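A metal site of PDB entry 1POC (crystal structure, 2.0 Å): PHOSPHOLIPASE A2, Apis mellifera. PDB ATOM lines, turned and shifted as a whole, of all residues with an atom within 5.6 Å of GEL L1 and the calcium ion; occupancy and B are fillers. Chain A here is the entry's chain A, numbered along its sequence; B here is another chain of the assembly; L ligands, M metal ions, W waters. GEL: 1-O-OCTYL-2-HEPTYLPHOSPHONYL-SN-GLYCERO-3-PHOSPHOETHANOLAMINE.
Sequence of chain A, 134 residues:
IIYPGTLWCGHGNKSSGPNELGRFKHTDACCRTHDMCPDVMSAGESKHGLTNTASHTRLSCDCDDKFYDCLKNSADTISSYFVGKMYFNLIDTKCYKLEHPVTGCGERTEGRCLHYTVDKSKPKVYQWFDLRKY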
ATOM      1  N   ILE A   1      12.983 -17.695  19.338  1.00  0.00           N
ATOM      2  CA  ILE A   1      11.523 -17.464  19.455  1.00  0.00           C
ATOM      3  C   ILE A   1      10.786 -18.659  18.828  1.00  0.00           C
ATOM      4  O   ILE A   1      11.145 -19.129  17.740  1.00  0.00           O
ATOM      5  CB  ILE A   1      11.173 -16.154  18.666  1.00  0.00           C
ATOM      6  CG1 ILE A   1       9.925 -15.456  19.213  1.00  0.00           C
ATOM      7  CG2 ILE A   1      10.914 -16.399  17.176  1.00  0.00           C
ATOM      8  CD1 ILE A   1       9.767 -15.622  20.728  1.00  0.00           C
ATOM      9  N   ILE A   2       9.791 -19.132  19.545  1.00  0.00           N
ATOM     10  CA  ILE A   2       8.899 -20.192  19.047  1.00  0.00           C
ATOM     11  C   ILE A   2       7.484 -19.622  19.071  1.00  0.00           C
ATOM     12  O   ILE A   2       7.071 -18.992  20.049  1.00  0.00           O
ATOM     13  CB  ILE A   2       9.030 -21.475  19.874  1.00  0.00           C
ATOM     14  CG1 ILE A   2      10.270 -22.297  19.493  1.00  0.00           C
ATOM     15  CG2 ILE A   2       7.851 -22.438  19.688  1.00  0.00           C
ATOM     16  CD1 ILE A   2      11.180 -22.599  20.691  1.00  0.00           C
ATOM     17  N   TYR A   3       6.798 -19.850  17.976  1.00  0.00           N
ATOM     18  CA  TYR A   3       5.415 -19.365  17.783  1.00  0.00           C
ATOM     19  C   TYR A   3       4.477 -20.134  18.714  1.00  0.00           C
ATOM     20  O   TYR A   3       4.333 -21.368  18.608  1.00  0.00           O
ATOM     21  CB  TYR A   3       5.035 -19.573  16.315  1.00  0.00           C
ATOM     22  CG  TYR A   3       3.593 -19.189  15.977  1.00  0.00           C
ATOM     23  CD1 TYR A   3       3.191 -17.841  16.037  1.00  0.00           C
ATOM     24  CD2 TYR A   3       2.679 -20.173  15.610  1.00  0.00           C
ATOM     25  CE1 TYR A   3       1.884 -17.495  15.704  1.00  0.00           C
ATOM     26  CE2 TYR A   3       1.371 -19.818  15.282  1.00  0.00           C
ATOM     27  CZ  TYR A   3       0.967 -18.485  15.325  1.00  0.00           C
ATOM     28  OH  TYR A   3      -0.307 -18.139  15.007  1.00  0.00           O
ATOM     29  N   TRP A   8       7.787 -26.462  17.500  1.00  0.00           N
ATOM     30  CA  TRP A   8       8.930 -26.498  16.568  1.00  0.00           C
ATOM     31  C   TRP A   8       9.075 -25.266  15.643  1.00  0.00           C
ATOM     32  O   TRP A   8      10.118 -25.063  15.003  1.00  0.00           O
ATOM     33  CB  TRP A   8       8.808 -27.711  15.640  1.00  0.00           C
ATOM     34  CG  TRP A   8       8.677 -29.045  16.392  1.00  0.00           C
ATOM     35  CD1 TRP A   8       7.570 -29.565  16.943  1.00  0.00           C
ATOM     36  CD2 TRP A   8       9.738 -29.960  16.627  1.00  0.00           C
ATOM     37  NE1 TRP A   8       7.932 -30.813  17.531  1.00  0.00           N
ATOM     38  CE2 TRP A   8       9.211 -31.031  17.342  1.00  0.00           C
ATOM     39  CE3 TRP A   8      11.106 -29.974  16.293  1.00  0.00           C
ATOM     40  CZ2 TRP A   8       9.972 -32.126  17.751  1.00  0.00           C
ATOM     41  CZ3 TRP A   8      11.865 -31.077  16.714  1.00  0.00           C
ATOM     42  CH2 TRP A   8      11.322 -32.109  17.415  1.00  0.00           C
ATOM     43  N   CYS A   9       8.046 -24.439  15.547  1.00  0.00           N
ATOM     44  CA  CYS A   9       8.102 -23.253  14.644  1.00  0.00           C
ATOM     45  C   CYS A   9       8.827 -22.078  15.324  1.00  0.00           C
ATOM     46  O   CYS A   9       8.262 -21.376  16.179  1.00  0.00           O
ATOM     47  CB  CYS A   9       6.698 -22.807  14.249  1.00  0.00           C
ATOM     48  SG  CYS A   9       5.765 -24.123  13.337  1.00  0.00           S
ATOM     49  N   GLY A  10      10.067 -21.899  14.893  1.00  0.00           N
ATOM     50  CA  GLY A  10      10.978 -20.841  15.402  1.00  0.00           C
ATOM     51  C   GLY A  10      12.373 -21.439  15.598  1.00  0.00           C
ATOM     52  O   GLY A  10      12.643 -22.571  15.172  1.00  0.00           O
ATOM     53  N   HIS A  11      13.244 -20.669  16.239  1.00  0.00           N
ATOM     54  CA  HIS A  11      14.627 -21.110  16.524  1.00  0.00           C
ATOM     55  C   HIS A  11      14.607 -22.365  17.378  1.00  0.00           C
ATOM     56  O   HIS A  11      14.164 -22.346  18.535  1.00  0.00           O
ATOM     57  CB  HIS A  11      15.390 -20.063  17.337  1.00  0.00           C
ATOM     58  CG  HIS A  11      15.444 -18.697  16.663  1.00  0.00           C
ATOM     59  ND1 HIS A  11      14.410 -17.781  16.791  1.00  0.00           N
ATOM     60  CD2 HIS A  11      16.382 -18.103  15.888  1.00  0.00           C
ATOM     61  CE1 HIS A  11      14.727 -16.703  16.112  1.00  0.00           C
ATOM     62  NE2 HIS A  11      15.906 -16.874  15.565  1.00  0.00           N
ATOM     63  N   GLY A  12      15.098 -23.435  16.792  1.00  0.00           N
ATOM     64  CA  GLY A  12      15.152 -24.741  17.448  1.00  0.00           C
ATOM     65  C   GLY A  12      13.735 -25.238  17.692  1.00  0.00           C
ATOM     66  O   GLY A  12      12.850 -25.104  16.825  1.00  0.00           O
ATOM     67  N   ASN A  13      13.550 -25.808  18.860  1.00  0.00           N
ATOM     68  CA  ASN A  13      12.258 -26.358  19.289  1.00  0.00           C
ATOM     69  C   ASN A  13      12.216 -26.397  20.818  1.00  0.00           C
ATOM     70  O   ASN A  13      13.260 -26.349  21.483  1.00  0.00           O
ATOM     71  CB  ASN A  13      12.111 -27.787  18.737  1.00  0.00           C
ATOM     72  CG  ASN A  13      12.972 -28.813  19.481  1.00  0.00           C
ATOM     73  OD1 ASN A  13      12.511 -29.410  20.452  1.00  0.00           O
ATOM     74  ND2 ASN A  13      14.202 -29.073  19.084  1.00  0.00           N
ATOM     75  N   CYS A  30       4.619 -29.541  10.111  1.00  0.00           N
ATOM     76  CA  CYS A  30       5.344 -29.011   8.956  1.00  0.00           C
ATOM     77  C   CYS A  30       6.719 -28.454   9.436  1.00  0.00           C
ATOM     78  O   CYS A  30       7.742 -28.606   8.752  1.00  0.00           O
ATOM     79  CB  CYS A  30       4.444 -27.977   8.243  1.00  0.00           C
ATOM     80  SG  CYS A  30       3.212 -28.789   7.129  1.00  0.00           S
ATOM     81  N   CYS A  31       6.730 -27.834  10.620  1.00  0.00           N
ATOM     82  CA  CYS A  31       7.973 -27.244  11.191  1.00  0.00           C
ATOM     83  C   CYS A  31       8.902 -28.326  11.767  1.00  0.00           C
ATOM     84  O   CYS A  31      10.133 -28.224  11.696  1.00  0.00           O
ATOM     85  CB  CYS A  31       7.641 -26.266  12.321  1.00  0.00           C
ATOM     86  SG  CYS A  31       6.762 -24.756  11.705  1.00  0.00           S
ATOM     87  N   HIS A  34      10.659 -29.871   9.006  1.00  0.00           N
ATOM     88  CA  HIS A  34      11.582 -28.822   8.525  1.00  0.00           C
ATOM     89  C   HIS A  34      12.867 -28.839   9.368  1.00  0.00           C
ATOM     90  O   HIS A  34      13.983 -28.827   8.839  1.00  0.00           O
ATOM     91  CB  HIS A  34      10.896 -27.448   8.617  1.00  0.00           C
ATOM     92  CG  HIS A  34      11.582 -26.359   7.770  1.00  0.00           C
ATOM     93  ND1 HIS A  34      11.747 -25.067   8.237  1.00  0.00           N
ATOM     94  CD2 HIS A  34      12.117 -26.385   6.519  1.00  0.00           C
ATOM     95  CE1 HIS A  34      12.359 -24.362   7.310  1.00  0.00           C
ATOM     96  NE2 HIS A  34      12.590 -25.125   6.276  1.00  0.00           N
ATOM     97  N   ASP A  35      12.663 -28.885  10.677  1.00  0.00           N
ATOM     98  CA  ASP A  35      13.763 -28.893  11.653  1.00  0.00           C
ATOM     99  C   ASP A  35      14.617 -30.170  11.527  1.00  0.00           C
ATOM    100  O   ASP A  35      15.809 -30.178  11.866  1.00  0.00           O
ATOM    101  CB  ASP A  35      13.211 -28.841  13.089  1.00  0.00           C
ATOM    102  CG  ASP A  35      12.904 -27.432  13.586  1.00  0.00           C
ATOM    103  OD1 ASP A  35      12.650 -26.481  12.757  1.00  0.00           O
ATOM    104  OD2 ASP A  35      12.898 -27.186  14.856  1.00  0.00           O
ATOM    105  N   MET A  36      13.978 -31.235  11.053  1.00  0.00           N
ATOM    106  CA  MET A  36      14.619 -32.565  10.945  1.00  0.00           C
ATOM    107  C   MET A  36      15.264 -32.783   9.564  1.00  0.00           C
ATOM    108  O   MET A  36      15.620 -33.916   9.204  1.00  0.00           O
ATOM    109  CB  MET A  36      13.589 -33.645  11.211  1.00  0.00           C
ATOM    110  CG  MET A  36      13.352 -33.845  12.707  1.00  0.00           C
ATOM    111  SD  MET A  36      12.051 -34.979  13.095  1.00  0.00           S
ATOM    112  CE  MET A  36      11.754 -34.934  14.845  1.00  0.00           C
ATOM    113  N   VAL A  40      21.461 -29.105   6.980  1.00  0.00           N
ATOM    114  CA  VAL A  40      21.284 -27.730   7.475  1.00  0.00           C
ATOM    115  C   VAL A  40      22.634 -27.185   7.943  1.00  0.00           C
ATOM    116  O   VAL A  40      23.567 -27.951   8.229  1.00  0.00           O
ATOM    117  CB  VAL A  40      20.382 -27.718   8.725  1.00  0.00           C
ATOM    118  CG1 VAL A  40      18.971 -28.265   8.451  1.00  0.00           C
ATOM    119  CG2 VAL A  40      20.934 -28.563   9.875  1.00  0.00           C
ATOM    120  N   HIS A  56      20.224 -17.120  12.106  1.00  0.00           N
ATOM    121  CA  HIS A  56      19.336 -18.297  12.163  1.00  0.00           C
ATOM    122  C   HIS A  56      19.835 -19.376  11.200  1.00  0.00           C
ATOM    123  O   HIS A  56      20.676 -19.116  10.328  1.00  0.00           O
ATOM    124  CB  HIS A  56      17.831 -17.950  11.907  1.00  0.00           C
ATOM    125  CG  HIS A  56      17.444 -17.160  10.634  1.00  0.00           C
ATOM    126  ND1 HIS A  56      17.201 -17.784   9.409  1.00  0.00           N
ATOM    127  CD2 HIS A  56      17.226 -15.832  10.405  1.00  0.00           C
ATOM    128  CE1 HIS A  56      16.848 -16.865   8.525  1.00  0.00           C
ATOM    129  NE2 HIS A  56      16.863 -15.695   9.107  1.00  0.00           N
ATOM    130  N   THR A  57      19.288 -20.556  11.408  1.00  0.00           N
ATOM    131  CA  THR A  57      19.627 -21.731  10.614  1.00  0.00           C
ATOM    132  C   THR A  57      19.126 -21.560   9.183  1.00  0.00           C
ATOM    133  O   THR A  57      18.055 -20.996   8.950  1.00  0.00           O
ATOM    134  CB  THR A  57      18.944 -22.976  11.188  1.00  0.00           C
ATOM    135  OG1 THR A  57      19.375 -23.206  12.521  1.00  0.00           O
ATOM    136  CG2 THR A  57      19.231 -24.252  10.383  1.00  0.00           C
ATOM    137  N   LEU A  59      18.793 -23.953   5.635  1.00  0.00           N
ATOM    138  CA  LEU A  59      18.799 -25.345   5.153  1.00  0.00           C
ATOM    139  C   LEU A  59      18.819 -25.443   3.632  1.00  0.00           C
ATOM    140  O   LEU A  59      18.697 -24.438   2.919  1.00  0.00           O
ATOM    141  CB  LEU A  59      17.548 -26.130   5.588  1.00  0.00           C
ATOM    142  CG  LEU A  59      16.558 -25.380   6.492  1.00  0.00           C
ATOM    143  CD1 LEU A  59      15.854 -26.325   7.477  1.00  0.00           C
ATOM    144  CD2 LEU A  59      17.198 -24.304   7.363  1.00  0.00           C
ATOM    145  N   PHE A  67       8.762 -27.712   2.889  1.00  0.00           N
ATOM    146  CA  PHE A  67       8.187 -26.920   3.986  1.00  0.00           C
ATOM    147  C   PHE A  67       7.074 -26.011   3.430  1.00  0.00           C
ATOM    148  O   PHE A  67       5.995 -25.863   4.025  1.00  0.00           O
ATOM    149  CB  PHE A  67       9.283 -26.072   4.635  1.00  0.00           C
ATOM    150  CG  PHE A  67       8.830 -25.324   5.897  1.00  0.00           C
ATOM    151  CD1 PHE A  67       8.052 -25.964   6.861  1.00  0.00           C
ATOM    152  CD2 PHE A  67       9.211 -23.981   6.090  1.00  0.00           C
ATOM    153  CE1 PHE A  67       7.636 -25.275   8.013  1.00  0.00           C
ATOM    154  CE2 PHE A  67       8.803 -23.288   7.238  1.00  0.00           C
ATOM    155  CZ  PHE A  67       8.014 -23.938   8.193  1.00  0.00           C
ATOM    156  N   PHE A  82       0.495 -17.451   8.680  1.00  0.00           N
ATOM    157  CA  PHE A  82       1.368 -16.538   9.447  1.00  0.00           C
ATOM    158  C   PHE A  82       2.825 -17.010   9.388  1.00  0.00           C
ATOM    159  O   PHE A  82       3.745 -16.221   9.137  1.00  0.00           O
ATOM    160  CB  PHE A  82       0.944 -16.444  10.909  1.00  0.00           C
ATOM    161  CG  PHE A  82       1.894 -15.559  11.724  1.00  0.00           C
ATOM    162  CD1 PHE A  82       1.768 -14.161  11.670  1.00  0.00           C
ATOM    163  CD2 PHE A  82       2.891 -16.143  12.511  1.00  0.00           C
ATOM    164  CE1 PHE A  82       2.655 -13.354  12.403  1.00  0.00           C
ATOM    165  CE2 PHE A  82       3.783 -15.338  13.227  1.00  0.00           C
ATOM    166  CZ  PHE A  82       3.664 -13.935  13.169  1.00  0.00           C
ATOM    167  N   VAL A  83       3.020 -18.290   9.624  1.00  0.00           N
ATOM    168  CA  VAL A  83       4.366 -18.891   9.626  1.00  0.00           C
ATOM    169  C   VAL A  83       4.950 -18.888   8.212  1.00  0.00           C
ATOM    170  O   VAL A  83       6.158 -18.695   8.023  1.00  0.00           O
ATOM    171  CB  VAL A  83       4.298 -20.318  10.187  1.00  0.00           C
ATOM    172  CG1 VAL A  83       5.607 -21.092   9.990  1.00  0.00           C
ATOM    173  CG2 VAL A  83       4.013 -20.357  11.684  1.00  0.00           C
ATOM    174  N   MET A  86       5.844 -15.174   7.128  1.00  0.00           N
ATOM    175  CA  MET A  86       7.015 -14.744   7.924  1.00  0.00           C
ATOM    176  C   MET A  86       8.320 -15.327   7.363  1.00  0.00           C
ATOM    177  O   MET A  86       9.275 -14.583   7.060  1.00  0.00           O
ATOM    178  CB  MET A  86       6.897 -15.212   9.372  1.00  0.00           C
ATOM    179  CG  MET A  86       5.956 -14.342  10.206  1.00  0.00           C
ATOM    180  SD  MET A  86       6.739 -12.858  10.812  1.00  0.00           S
ATOM    181  CE  MET A  86       8.483 -13.138  10.973  1.00  0.00           C
ATOM    182  N   TYR A  87       8.330 -16.638   7.236  1.00  0.00           N
ATOM    183  CA  TYR A  87       9.530 -17.387   6.807  1.00  0.00           C
ATOM    184  C   TYR A  87       9.941 -17.127   5.349  1.00  0.00           C
ATOM    185  O   TYR A  87      11.119 -16.878   5.061  1.00  0.00           O
ATOM    186  CB  TYR A  87       9.297 -18.906   6.933  1.00  0.00           C
ATOM    187  CG  TYR A  87      10.573 -19.718   6.682  1.00  0.00           C
ATOM    188  CD1 TYR A  87      11.542 -19.823   7.691  1.00  0.00           C
ATOM    189  CD2 TYR A  87      10.777 -20.347   5.446  1.00  0.00           C
ATOM    190  CE1 TYR A  87      12.707 -20.547   7.460  1.00  0.00           C
ATOM    191  CE2 TYR A  87      11.947 -21.074   5.223  1.00  0.00           C
ATOM    192  CZ  TYR A  87      12.916 -21.179   6.232  1.00  0.00           C
ATOM    193  OH  TYR A  87      14.063 -21.887   6.006  1.00  0.00           O
ATOM    194  N   ILE A  91      11.571 -12.636   6.543  1.00  0.00           N
ATOM    195  CA  ILE A  91      12.899 -12.745   7.208  1.00  0.00           C
ATOM    196  C   ILE A  91      14.079 -12.734   6.228  1.00  0.00           C
ATOM    197  O   ILE A  91      15.248 -12.687   6.627  1.00  0.00           O
ATOM    198  CB  ILE A  91      12.992 -14.005   8.082  1.00  0.00           C
ATOM    199  CG1 ILE A  91      12.790 -15.302   7.297  1.00  0.00           C
ATOM    200  CG2 ILE A  91      11.962 -14.010   9.213  1.00  0.00           C
ATOM    201  CD1 ILE A  91      13.204 -16.540   8.092  1.00  0.00           C
ATOM    202  N   PHE B  82       5.756 -13.160  23.169  1.00  0.00           N
ATOM    203  CA  PHE B  82       6.117 -13.414  21.759  1.00  0.00           C
ATOM    204  C   PHE B  82       6.247 -12.094  20.990  1.00  0.00           C
ATOM    205  O   PHE B  82       7.217 -11.872  20.255  1.00  0.00           O
ATOM    206  CB  PHE B  82       5.083 -14.288  21.057  1.00  0.00           C
ATOM    207  CG  PHE B  82       5.414 -14.487  19.574  1.00  0.00           C
ATOM    208  CD1 PHE B  82       6.374 -15.440  19.193  1.00  0.00           C
ATOM    209  CD2 PHE B  82       4.770 -13.714  18.603  1.00  0.00           C
ATOM    210  CE1 PHE B  82       6.689 -15.605  17.834  1.00  0.00           C
ATOM    211  CE2 PHE B  82       5.096 -13.869  17.252  1.00  0.00           C
ATOM    212  CZ  PHE B  82       6.064 -14.818  16.867  1.00  0.00           C
ATOM    213  N   MET B  86       9.878 -10.376  19.783  1.00  0.00           N
ATOM    214  CA  MET B  86       9.973 -10.129  18.327  1.00  0.00           C
ATOM    215  C   MET B  86      10.319  -8.664  18.027  1.00  0.00           C
ATOM    216  O   MET B  86      11.303  -8.371  17.319  1.00  0.00           O
ATOM    217  CB  MET B  86       8.649 -10.432  17.631  1.00  0.00           C
ATOM    218  CG  MET B  86       8.420 -11.927  17.407  1.00  0.00           C
ATOM    219  SD  MET B  86       9.255 -12.547  15.957  1.00  0.00           S
ATOM    220  CE  MET B  86       9.450 -11.230  14.785  1.00  0.00           C
ATOM    221  N   LEU B  90      14.264  -9.004  18.065  1.00  0.00           N
ATOM    222  CA  LEU B  90      14.572  -9.694  16.798  1.00  0.00           C
ATOM    223  C   LEU B  90      14.487  -8.861  15.504  1.00  0.00           C
ATOM    224  O   LEU B  90      15.199  -9.121  14.520  1.00  0.00           O
ATOM    225  CB  LEU B  90      13.642 -10.909  16.642  1.00  0.00           C
ATOM    226  CG  LEU B  90      13.849 -11.955  17.738  1.00  0.00           C
ATOM    227  CD1 LEU B  90      12.826 -13.092  17.675  1.00  0.00           C
ATOM    228  CD2 LEU B  90      15.222 -12.629  17.670  1.00  0.00           C
ATOM    229  N   ILE B  91      13.639  -7.844  15.422  1.00  0.00           N
ATOM    230  CA  ILE B  91      13.496  -7.101  14.138  1.00  0.00           C
ATOM    231  C   ILE B  91      14.496  -5.947  13.982  1.00  0.00           C
ATOM    232  O   ILE B  91      14.593  -5.318  12.923  1.00  0.00           O
ATOM    233  CB  ILE B  91      12.073  -6.552  13.957  1.00  0.00           C
ATOM    234  CG1 ILE B  91      11.653  -5.597  15.064  1.00  0.00           C
ATOM    235  CG2 ILE B  91      11.020  -7.661  13.913  1.00  0.00           C
ATOM    236  CD1 ILE B  91      10.387  -4.804  14.717  1.00  0.00           C
HETATM  237  C1  GEL L   1      14.692 -21.904  10.665  1.00  0.00           C
HETATM  238  O1  GEL L   1      13.922 -20.670  10.717  1.00  0.00           O
HETATM  239  C11 GEL L   1      14.565 -19.847  11.740  1.00  0.00           C
HETATM  240  C12 GEL L   1      13.572 -18.854  12.337  1.00  0.00           C
HETATM  241  C13 GEL L   1      14.046 -17.418  12.420  1.00  0.00           C
HETATM  242  C14 GEL L   1      13.153 -16.459  13.175  1.00  0.00           C
HETATM  243  C15 GEL L   1      13.097 -15.070  12.624  1.00  0.00           C
HETATM  244  C16 GEL L   1      12.861 -13.921  13.541  1.00  0.00           C
HETATM  245  C17 GEL L   1      13.195 -12.552  13.000  1.00  0.00           C
HETATM  246  C18 GEL L   1      12.081 -11.509  13.178  1.00  0.00           C
HETATM  247  C2  GEL L   1      13.885 -23.031  11.241  1.00  0.00           C
HETATM  248  O2  GEL L   1      12.577 -23.005  10.698  1.00  0.00           O
HETATM  249  P2  GEL L   1      11.180 -23.368  11.405  1.00  0.00           P
HETATM  250  O1P GEL L   1      10.611 -24.478  10.587  1.00  0.00           O
HETATM  251  O2P GEL L   1      11.394 -23.698  12.819  1.00  0.00           O
HETATM  252  C22 GEL L   1      10.758 -21.679  10.961  1.00  0.00           C
HETATM  253  C23 GEL L   1       9.720 -20.867  11.527  1.00  0.00           C
HETATM  254  C24 GEL L   1       9.684 -19.360  11.422  1.00  0.00           C
HETATM  255  C25 GEL L   1       8.342 -18.857  11.854  1.00  0.00           C
HETATM  256  C26 GEL L   1       8.079 -17.580  12.491  1.00  0.00           C
HETATM  257  C27 GEL L   1       7.304 -17.587  13.797  1.00  0.00           C
HETATM  258  C28 GEL L   1       8.129 -16.934  14.901  1.00  0.00           C
HETATM  259  C3  GEL L   1      14.545 -24.384  11.074  1.00  0.00           C
HETATM  260  O3  GEL L   1      15.800 -24.337  11.781  1.00  0.00           O
HETATM  261  P3  GEL L   1      15.906 -24.800  13.352  1.00  0.00           P
HETATM  262  O3P GEL L   1      17.058 -24.030  13.910  1.00  0.00           O
HETATM  263  O4P GEL L   1      14.641 -24.626  14.049  1.00  0.00           O
HETATM  264  O5P GEL L   1      16.307 -26.198  12.856  1.00  0.00           O
HETATM  265  C31 GEL L   1      16.430 -27.411  13.547  1.00  0.00           C
HETATM  266  C32 GEL L   1      17.845 -27.946  13.345  1.00  0.00           C
HETATM  267  N3  GEL L   1      18.310 -28.332  14.727  1.00  0.00           N
HETATM  268  C1  GEL L   2       5.405  -1.308  13.965  1.00  0.00           C
HETATM  269  O1  GEL L   2       5.999  -2.636  14.005  1.00  0.00           O
HETATM  270  C11 GEL L   2       6.061  -3.082  12.614  1.00  0.00           C
HETATM  271  C12 GEL L   2       6.061  -4.606  12.535  1.00  0.00           C
HETATM  272  C13 GEL L   2       7.126  -5.220  11.650  1.00  0.00           C
HETATM  273  C14 GEL L   2       7.025  -6.710  11.413  1.00  0.00           C
HETATM  274  C15 GEL L   2       8.331  -7.431  11.312  1.00  0.00           C
HETATM  275  C16 GEL L   2       8.438  -8.649  10.463  1.00  0.00           C
HETATM  276  C17 GEL L   2       9.835  -9.093  10.101  1.00  0.00           C
HETATM  277  C18 GEL L   2      10.116 -10.581  10.358  1.00  0.00           C
HETATM  278  C2  GEL L   2       4.017  -1.354  14.534  1.00  0.00           C
HETATM  279  O2  GEL L   2       4.027  -2.074  15.753  1.00  0.00           O
HETATM  280  P2  GEL L   2       2.907  -3.055  16.358  1.00  0.00           P
HETATM  281  O1P GEL L   2       2.532  -2.451  17.669  1.00  0.00           O
HETATM  282  O2P GEL L   2       1.796  -3.205  15.413  1.00  0.00           O
HETATM  283  C22 GEL L   2       4.243  -4.256  16.325  1.00  0.00           C
HETATM  284  C23 GEL L   2       4.127  -5.685  16.361  1.00  0.00           C
HETATM  285  C24 GEL L   2       5.221  -6.627  15.915  1.00  0.00           C
HETATM  286  C25 GEL L   2       4.896  -8.020  16.352  1.00  0.00           C
HETATM  287  C26 GEL L   2       5.271  -9.238  15.657  1.00  0.00           C
HETATM  288  C27 GEL L   2       4.171 -10.232  15.328  1.00  0.00           C
HETATM  289  C28 GEL L   2       4.115 -10.475  13.823  1.00  0.00           C
HETATM  290  C3  GEL L   2       3.389   0.016  14.684  1.00  0.00           C
HETATM  291  O3  GEL L   2       3.304   0.594  13.367  1.00  0.00           O
HETATM  292  P3  GEL L   2       1.964   0.398  12.440  1.00  0.00           P
HETATM  293  O3P GEL L   2       2.447   0.501  11.029  1.00  0.00           O
HETATM  294  O4P GEL L   2       1.257  -0.829  12.770  1.00  0.00           O
HETATM  295  O5P GEL L   2       1.451   1.736  12.994  1.00  0.00           O
HETATM  296  C31 GEL L   2       0.190   2.341  12.896  1.00  0.00           C
HETATM  297  C32 GEL L   2       0.361   3.723  12.271  1.00  0.00           C
HETATM  298  N3  GEL L   2      -0.697   3.793  11.198  1.00  0.00           N
HETATM  299 CA    CA M   1      12.406 -24.857  14.528  1.00  0.00          CA
HETATM  300  O   HOH W   1      14.769 -27.834  16.415  1.00  0.00           O
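An oxygen (O2P) of GEL L1 lies close to the backbone NH (N) of Gly 10 (3.0 Å).
The side-chain hydroxyl (OG1) of Thr 57 is in hydrogen-bond range of an oxygen (O3P) of GEL L1, at 2.8 Å.
A ring nitrogen (ND1) of His 34 lies within hydrogen-bond range of an oxygen (O1P) of GEL L1, 2.7 Å away.
An oxygen (O4P) of GEL L1 lies close to the backbone NH (N) of Gly 12.
The backbone NH (N) of Ile 91 of chain A sits at hydrogen-bond distance from the backbone carbonyl oxygen (O) of Met 86 of chain A, at 3.1 Å.
A ring nitrogen (ND1) of His 11 is in hydrogen-bond range of the backbone NH of Ile 1, at 2.9 Å.
O of Met 86 of chain B lies within hydrogen-bond range of N of Ile 91 of chain B (3.1 Å).
SG of Cys 9 forms a disulfide with SG of Cys 31.
O of Cys 9 sits at hydrogen-bond distance from N of Tyr 3, at 2.8 Å.
Ile 1 touches GEL L1 (CG2 to C28, 3.6 Å).
Tyr 3 touches GEL L1.
CA of Cys 9 touches O2P of GEL L1, 3.8 Å away.
CE1 of His 11 touches C14 of GEL L1, 3.3 Å away.
Cys 31 touches GEL L1 (CA to O1P, 3.9 Å).
His 56 touches GEL L1 (CB to C11, 3.8 Å).
Phe 67 touches GEL L1.
Val 83 touches GEL L1 (CG1 to C25, 3.99 Å).
CE1 of Tyr 87 touches O1 of GEL L1 (3.5 Å).
Ile 91 of chain A touches GEL L1 (CG2 to C15, 3.7 Å).
Phe 82 of chain B touches GEL L1.
CE of Met 86 of chain B touches C18 of GEL L1, 3.1 Å away.
Leu 90 of chain B touches GEL L1 (CB to C18, 3.8 Å).
Hydrophobic or aromatic side chains within 4 Å of GEL L1: Ile 1, Tyr 3, His 11, His 34, His 56, Phe 67, Val 83, Tyr 87, Ile 91 of chain A, Phe 82 of chain B, Met 86 of chain B and Leu 90 of chain B.
Of the 28 residues printed, 19 come within 4 Å of GEL L1.
The calcium ion is bound by an oxygen (O4P) of GEL L1 (2.3 Å), an oxygen (O2P) of GEL L1 (2.3 Å), the backbone carbonyl oxygen (O) of Trp 8 (2.3 Å), the backbone carbonyl oxygen (O) of Gly 12 (2.4 Å), the backbone carbonyl oxygen (O) of Gly 10 (2.4 Å), the side-chain carboxylate (OD2) of Asp 35 (2.4 Å) and the side-chain carboxylate (OD1) of Asp 35 (2.4 Å).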
